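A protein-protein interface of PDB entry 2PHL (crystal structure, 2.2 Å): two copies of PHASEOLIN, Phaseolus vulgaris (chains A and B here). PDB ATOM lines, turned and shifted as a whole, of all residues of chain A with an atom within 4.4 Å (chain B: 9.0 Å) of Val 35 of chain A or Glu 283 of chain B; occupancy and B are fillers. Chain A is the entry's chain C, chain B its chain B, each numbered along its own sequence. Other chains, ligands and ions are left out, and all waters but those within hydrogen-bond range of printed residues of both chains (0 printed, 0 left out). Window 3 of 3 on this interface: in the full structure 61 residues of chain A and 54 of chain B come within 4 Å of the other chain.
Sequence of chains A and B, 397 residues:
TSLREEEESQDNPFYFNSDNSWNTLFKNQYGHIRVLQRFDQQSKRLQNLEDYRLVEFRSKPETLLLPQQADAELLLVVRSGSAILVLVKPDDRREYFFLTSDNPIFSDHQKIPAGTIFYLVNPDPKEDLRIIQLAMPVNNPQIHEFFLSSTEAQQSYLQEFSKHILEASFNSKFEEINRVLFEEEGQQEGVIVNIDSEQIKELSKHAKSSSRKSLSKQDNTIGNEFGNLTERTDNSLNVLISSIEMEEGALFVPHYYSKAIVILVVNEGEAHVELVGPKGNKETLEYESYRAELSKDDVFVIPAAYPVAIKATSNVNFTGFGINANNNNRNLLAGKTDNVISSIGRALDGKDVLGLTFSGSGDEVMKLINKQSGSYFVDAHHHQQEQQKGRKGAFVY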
ATOM      1  N   SER A  21       6.194   7.435  35.023  1.00  0.00           N
ATOM      2  CA  SER A  21       7.477   8.120  34.986  1.00  0.00           C
ATOM      3  C   SER A  21       8.723   7.269  34.821  1.00  0.00           C
ATOM      4  O   SER A  21       9.775   7.795  34.420  1.00  0.00           O
ATOM      5  CB  SER A  21       7.628   8.988  36.211  1.00  0.00           C
ATOM      6  OG  SER A  21       6.592   9.955  36.254  1.00  0.00           O
ATOM      7  N   TRP A  22       8.613   5.975  35.137  1.00  0.00           N
ATOM      8  CA  TRP A  22       9.726   5.021  35.032  1.00  0.00           C
ATOM      9  C   TRP A  22       9.560   4.137  33.796  1.00  0.00           C
ATOM     10  O   TRP A  22       8.447   3.730  33.495  1.00  0.00           O
ATOM     11  CB  TRP A  22       9.741   4.102  36.260  1.00  0.00           C
ATOM     12  CG  TRP A  22      10.004   4.799  37.546  1.00  0.00           C
ATOM     13  CD1 TRP A  22       9.081   5.291  38.414  1.00  0.00           C
ATOM     14  CD2 TRP A  22      11.295   5.113  38.097  1.00  0.00           C
ATOM     15  NE1 TRP A  22       9.715   5.907  39.469  1.00  0.00           N
ATOM     16  CE2 TRP A  22      11.074   5.816  39.295  1.00  0.00           C
ATOM     17  CE3 TRP A  22      12.617   4.872  37.681  1.00  0.00           C
ATOM     18  CZ2 TRP A  22      12.129   6.286  40.100  1.00  0.00           C
ATOM     19  CZ3 TRP A  22      13.671   5.344  38.483  1.00  0.00           C
ATOM     20  CH2 TRP A  22      13.415   6.047  39.676  1.00  0.00           C
ATOM     21  N   ASN A  23      10.636   3.836  33.077  1.00  0.00           N
ATOM     22  CA  ASN A  23      10.518   2.957  31.918  1.00  0.00           C
ATOM     23  C   ASN A  23      11.386   1.750  32.205  1.00  0.00           C
ATOM     24  O   ASN A  23      12.520   1.916  32.625  1.00  0.00           O
ATOM     25  CB  ASN A  23      10.995   3.661  30.650  1.00  0.00           C
ATOM     26  CG  ASN A  23      10.098   4.839  30.243  1.00  0.00           C
ATOM     27  OD1 ASN A  23       9.149   4.676  29.469  1.00  0.00           O
ATOM     28  ND2 ASN A  23      10.420   6.035  30.731  1.00  0.00           N
ATOM     29  N   LEU A  25      13.930  -1.210  31.738  1.00  0.00           N
ATOM     30  CA  LEU A  25      15.041  -1.575  30.881  1.00  0.00           C
ATOM     31  C   LEU A  25      15.146  -3.094  30.767  1.00  0.00           C
ATOM     32  O   LEU A  25      15.389  -3.632  29.693  1.00  0.00           O
ATOM     33  CB  LEU A  25      16.327  -1.016  31.465  1.00  0.00           C
ATOM     34  CG  LEU A  25      17.328  -0.354  30.528  1.00  0.00           C
ATOM     35  CD1 LEU A  25      18.688  -0.882  30.883  1.00  0.00           C
ATOM     36  CD2 LEU A  25      17.032  -0.646  29.080  1.00  0.00           C
ATOM     37  N   ARG A  34      14.964  -0.068  36.137  1.00  0.00           N
ATOM     38  CA  ARG A  34      14.124   0.989  35.573  1.00  0.00           C
ATOM     39  C   ARG A  34      14.930   2.291  35.491  1.00  0.00           C
ATOM     40  O   ARG A  34      15.849   2.524  36.284  1.00  0.00           O
ATOM     41  CB  ARG A  34      12.852   1.221  36.414  1.00  0.00           C
ATOM     42  CG  ARG A  34      11.673   0.383  35.974  1.00  0.00           C
ATOM     43  CD  ARG A  34      10.956  -0.280  37.137  1.00  0.00           C
ATOM     44  NE  ARG A  34      10.053   0.631  37.822  1.00  0.00           N
ATOM     45  CZ  ARG A  34       9.567   0.423  39.042  1.00  0.00           C
ATOM     46  NH1 ARG A  34       9.907  -0.673  39.717  1.00  0.00           N
ATOM     47  NH2 ARG A  34       8.760   1.323  39.599  1.00  0.00           N
ATOM     48  N   VAL A  35      14.572   3.131  34.531  1.00  0.00           N
ATOM     49  CA  VAL A  35      15.221   4.411  34.309  1.00  0.00           C
ATOM     50  C   VAL A  35      14.119   5.488  34.358  1.00  0.00           C
ATOM     51  O   VAL A  35      13.053   5.282  33.772  1.00  0.00           O
ATOM     52  CB  VAL A  35      15.908   4.384  32.918  1.00  0.00           C
ATOM     53  CG1 VAL A  35      16.714   5.660  32.661  1.00  0.00           C
ATOM     54  CG2 VAL A  35      16.813   3.172  32.834  1.00  0.00           C
ATOM     55  N   LEU A  36      14.327   6.573  35.116  1.00  0.00           N
ATOM     56  CA  LEU A  36      13.322   7.654  35.195  1.00  0.00           C
ATOM     57  C   LEU A  36      13.332   8.538  33.918  1.00  0.00           C
ATOM     58  O   LEU A  36      14.357   8.673  33.232  1.00  0.00           O
ATOM     59  CB  LEU A  36      13.520   8.545  36.453  1.00  0.00           C
ATOM     60  CG  LEU A  36      12.387   9.551  36.808  1.00  0.00           C
ATOM     61  CD1 LEU A  36      11.200   8.854  37.438  1.00  0.00           C
ATOM     62  CD2 LEU A  36      12.862  10.683  37.725  1.00  0.00           C
ATOM     63  N   GLN A  37      12.171   9.085  33.567  1.00  0.00           N
ATOM     64  CA  GLN A  37      12.081   9.935  32.398  1.00  0.00           C
ATOM     65  C   GLN A  37      12.946  11.183  32.634  1.00  0.00           C
ATOM     66  O   GLN A  37      13.197  11.546  33.784  1.00  0.00           O
ATOM     67  CB  GLN A  37      10.621  10.320  32.119  1.00  0.00           C
ATOM     68  CG  GLN A  37       9.992  11.261  33.125  1.00  0.00           C
ATOM     69  CD  GLN A  37       8.874  12.107  32.517  1.00  0.00           C
ATOM     70  OE1 GLN A  37       9.146  13.055  31.777  1.00  0.00           O
ATOM     71  NE2 GLN A  37       7.616  11.763  32.811  1.00  0.00           N
ATOM     72  N   ARG A  53      20.148  11.923  35.970  1.00  0.00           N
ATOM     73  CA  ARG A  53      19.143  10.873  35.845  1.00  0.00           C
ATOM     74  C   ARG A  53      19.058   9.977  37.064  1.00  0.00           C
ATOM     75  O   ARG A  53      19.955   9.981  37.900  1.00  0.00           O
ATOM     76  CB  ARG A  53      19.491  10.001  34.642  1.00  0.00           C
ATOM     77  CG  ARG A  53      19.251  10.628  33.276  1.00  0.00           C
ATOM     78  CD  ARG A  53      17.763  10.647  32.908  1.00  0.00           C
ATOM     79  NE  ARG A  53      17.608  10.342  31.503  1.00  0.00           N
ATOM     80  CZ  ARG A  53      16.931   9.308  31.044  1.00  0.00           C
ATOM     81  NH1 ARG A  53      16.319   8.500  31.892  1.00  0.00           N
ATOM     82  NH2 ARG A  53      16.965   9.012  29.752  1.00  0.00           N
ATOM     83  N   LEU A  54      17.972   9.217  37.167  1.00  0.00           N
ATOM     84  CA  LEU A  54      17.806   8.275  38.272  1.00  0.00           C
ATOM     85  C   LEU A  54      17.587   6.874  37.725  1.00  0.00           C
ATOM     86  O   LEU A  54      16.857   6.681  36.757  1.00  0.00           O
ATOM     87  CB  LEU A  54      16.604   8.624  39.171  1.00  0.00           C
ATOM     88  CG  LEU A  54      16.503   9.921  39.994  1.00  0.00           C
ATOM     89  CD1 LEU A  54      15.201   9.855  40.778  1.00  0.00           C
ATOM     90  CD2 LEU A  54      17.687  10.165  40.946  1.00  0.00           C
ATOM     91  N   GLN A 142      21.030  10.680  27.334  1.00  0.00           N
ATOM     92  CA  GLN A 142      20.669   9.275  27.487  1.00  0.00           C
ATOM     93  C   GLN A 142      21.753   8.547  28.247  1.00  0.00           C
ATOM     94  O   GLN A 142      22.934   8.846  28.075  1.00  0.00           O
ATOM     95  CB  GLN A 142      20.511   8.596  26.121  1.00  0.00           C
ATOM     96  CG  GLN A 142      19.132   8.694  25.497  1.00  0.00           C
ATOM     97  CD  GLN A 142      18.564  10.085  25.538  1.00  0.00           C
ATOM     98  OE1 GLN A 142      19.162  11.037  25.030  1.00  0.00           O
ATOM     99  NE2 GLN A 142      17.402  10.222  26.160  1.00  0.00           N
ATOM    100  N   ILE A 143      21.344   7.561  29.042  1.00  0.00           N
ATOM    101  CA  ILE A 143      22.269   6.728  29.811  1.00  0.00           C
ATOM    102  C   ILE A 143      22.330   5.378  29.068  1.00  0.00           C
ATOM    103  O   ILE A 143      21.292   4.804  28.754  1.00  0.00           O
ATOM    104  CB  ILE A 143      21.821   6.592  31.343  1.00  0.00           C
ATOM    105  CG1 ILE A 143      22.420   5.355  32.012  1.00  0.00           C
ATOM    106  CG2 ILE A 143      20.337   6.484  31.473  1.00  0.00           C
ATOM    107  CD1 ILE A 143      23.916   5.390  32.225  1.00  0.00           C
ATOM    108  N   ARG B  45      23.045  13.613  18.982  1.00  0.00           N
ATOM    109  CA  ARG B  45      23.687  12.552  19.758  1.00  0.00           C
ATOM    110  C   ARG B  45      25.099  12.987  20.093  1.00  0.00           C
ATOM    111  O   ARG B  45      25.801  12.347  20.886  1.00  0.00           O
ATOM    112  CB  ARG B  45      23.799  11.289  18.922  1.00  0.00           C
ATOM    113  CG  ARG B  45      22.495  10.710  18.488  1.00  0.00           C
ATOM    114  CD  ARG B  45      22.745   9.664  17.427  1.00  0.00           C
ATOM    115  NE  ARG B  45      23.176   8.404  17.999  1.00  0.00           N
ATOM    116  CZ  ARG B  45      22.742   7.225  17.578  1.00  0.00           C
ATOM    117  NH1 ARG B  45      21.883   7.160  16.568  1.00  0.00           N
ATOM    118  NH2 ARG B  45      23.078   6.121  18.238  1.00  0.00           N
ATOM    119  N   PRO B 278      24.637   2.325  20.753  1.00  0.00           N
ATOM    120  CA  PRO B 278      23.255   1.932  21.055  1.00  0.00           C
ATOM    121  C   PRO B 278      22.437   2.004  19.760  1.00  0.00           C
ATOM    122  O   PRO B 278      22.678   2.870  18.919  1.00  0.00           O
ATOM    123  CB  PRO B 278      22.821   2.995  22.058  1.00  0.00           C
ATOM    124  CG  PRO B 278      23.549   4.221  21.570  1.00  0.00           C
ATOM    125  CD  PRO B 278      24.927   3.674  21.278  1.00  0.00           C
ATOM    126  N   LYS B 279      21.518   1.062  19.581  1.00  0.00           N
ATOM    127  CA  LYS B 279      20.684   1.011  18.394  1.00  0.00           C
ATOM    128  C   LYS B 279      19.801   2.249  18.330  1.00  0.00           C
ATOM    129  O   LYS B 279      18.670   2.237  18.830  1.00  0.00           O
ATOM    130  CB  LYS B 279      19.824  -0.244  18.427  1.00  0.00           C
ATOM    131  CG  LYS B 279      18.931  -0.400  17.231  1.00  0.00           C
ATOM    132  CD  LYS B 279      18.026  -1.600  17.394  1.00  0.00           C
ATOM    133  CE  LYS B 279      16.727  -1.419  16.618  1.00  0.00           C
ATOM    134  NZ  LYS B 279      15.895  -0.290  17.150  1.00  0.00           N
ATOM    135  N   GLY B 280      20.330   3.323  17.743  1.00  0.00           N
ATOM    136  CA  GLY B 280      19.589   4.571  17.632  1.00  0.00           C
ATOM    137  C   GLY B 280      19.768   5.477  18.843  1.00  0.00           C
ATOM    138  O   GLY B 280      19.040   6.460  19.031  1.00  0.00           O
ATOM    139  N   GLU B 283      17.213   3.958  24.283  1.00  0.00           N
ATOM    140  CA  GLU B 283      17.448   3.468  25.640  1.00  0.00           C
ATOM    141  C   GLU B 283      16.985   2.022  25.829  1.00  0.00           C
ATOM    142  O   GLU B 283      15.953   1.781  26.450  1.00  0.00           O
ATOM    143  CB  GLU B 283      16.743   4.374  26.645  1.00  0.00           C
ATOM    144  CG  GLU B 283      17.587   4.716  27.855  1.00  0.00           C
ATOM    145  CD  GLU B 283      17.203   6.052  28.456  1.00  0.00           C
ATOM    146  OE1 GLU B 283      16.230   6.084  29.244  1.00  0.00           O
ATOM    147  OE2 GLU B 283      17.870   7.061  28.130  1.00  0.00           O
ATOM    148  N   THR B 284      17.763   1.080  25.285  1.00  0.00           N
ATOM    149  CA  THR B 284      17.491  -0.366  25.336  1.00  0.00           C
ATOM    150  C   THR B 284      18.816  -1.120  25.427  1.00  0.00           C
ATOM    151  O   THR B 284      19.880  -0.517  25.530  1.00  0.00           O
ATOM    152  CB  THR B 284      16.774  -0.889  24.041  1.00  0.00           C
ATOM    153  OG1 THR B 284      17.571  -0.589  22.881  1.00  0.00           O
ATOM    154  CG2 THR B 284      15.369  -0.298  23.889  1.00  0.00           C
ATOM    155  N   LEU B 285      18.749  -2.440  25.344  1.00  0.00           N
ATOM    156  CA  LEU B 285      19.950  -3.270  25.402  1.00  0.00           C
ATOM    157  C   LEU B 285      20.180  -3.834  24.004  1.00  0.00           C
ATOM    158  O   LEU B 285      20.639  -4.967  23.845  1.00  0.00           O
ATOM    159  CB  LEU B 285      19.751  -4.431  26.387  1.00  0.00           C
ATOM    160  CG  LEU B 285      19.113  -4.140  27.738  1.00  0.00           C
ATOM    161  CD1 LEU B 285      19.055  -5.432  28.550  1.00  0.00           C
ATOM    162  CD2 LEU B 285      19.914  -3.075  28.466  1.00  0.00           C
ATOM    163  N   GLU B 286      19.840  -3.048  22.988  1.00  0.00           N
ATOM    164  CA  GLU B 286      19.996  -3.501  21.608  1.00  0.00           C
ATOM    165  C   GLU B 286      21.088  -2.695  20.935  1.00  0.00           C
ATOM    166  O   GLU B 286      21.023  -1.471  20.912  1.00  0.00           O
ATOM    167  CB  GLU B 286      18.668  -3.351  20.862  1.00  0.00           C
ATOM    168  CG  GLU B 286      18.438  -4.382  19.760  1.00  0.00           C
ATOM    169  CD  GLU B 286      16.974  -4.512  19.375  1.00  0.00           C
ATOM    170  OE1 GLU B 286      16.104  -4.309  20.252  1.00  0.00           O
ATOM    171  OE2 GLU B 286      16.695  -4.836  18.202  1.00  0.00           O
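The guanidinium group (NH2) of Arg 53 of chain A is in salt-bridge range of the side-chain carboxylate (OE2) of Glu 283 of chain B (2.7 Å).
No position is printed for both chains.
Of the 7 pairs that touch across the chains among the printed residues, none has its exchanged pair printed and touching as well.
Of the 12 printed residues of chain A, 5 touch a printed residue of chain B.
Hydrophobic or aromatic side chains of chain A that line the printed part of chain B: Leu 25 and Val 35.
Of the 8 printed residues of chain B, 3 touch a printed residue of chain A.
Among the printed residues, Asp or Glu carboxylates within 4 Å of a Lys or Arg side-chain nitrogen of the other chain: Arg 53 of chain A with Glu 283 of chain B.
CD2 of Leu 25 of chain A touches O of Glu 283 of chain B, at 3.7 Å.
Leu 25 of chain A touches Thr 284 of chain B (CD2 to CA, 3.8 Å).
Leu 25 of chain A touches Leu 285 of chain B (CD1 to CD2, 3.5 Å).
Glu 283 of chain B touches Val 35 of chain A.
Gln 142 of chain A touches Glu 283 of chain B (CG to OE2, 3.3 Å).
Ile 143 of chain A touches Glu 283 of chain B.
The side-chain hydroxyl (OG1) of Thr 284 of chain B lies close to the backbone NH (N) of Glu 286 of chain B, at 3.3 Å.
N of Asn 23 of chain A is in hydrogen-bond range of O of Val 35 of chain A, 2.9 Å away.
Val 35 of chain A touches just one residue of chain B: Glu 283.
Printed residues of chain A within 4 Å of Glu 283 of chain B: Leu 25 (3.7 Å), Val 35 (3.5 Å), Arg 53 (2.7 Å), Gln 142 (3.3 Å) and Ile 143 (3.6 Å).
Of the printed residues of chain B, Arg 53 of chain A touches Glu 283.
Of the printed residues of chain A, Leu 285 of chain B touches Leu 25.
Of the printed residues of chain B, Gln 142 of chain A touches Glu 283 (3.3 Å).
Of the printed residues of chain A, Thr 284 of chain B touches Leu 25.
Of the printed residues of chain B, Leu 25 of chain A touches Glu 283, Thr 284 and Leu 285.
Pro 278 of chain B touches none of the printed residues of chain A.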
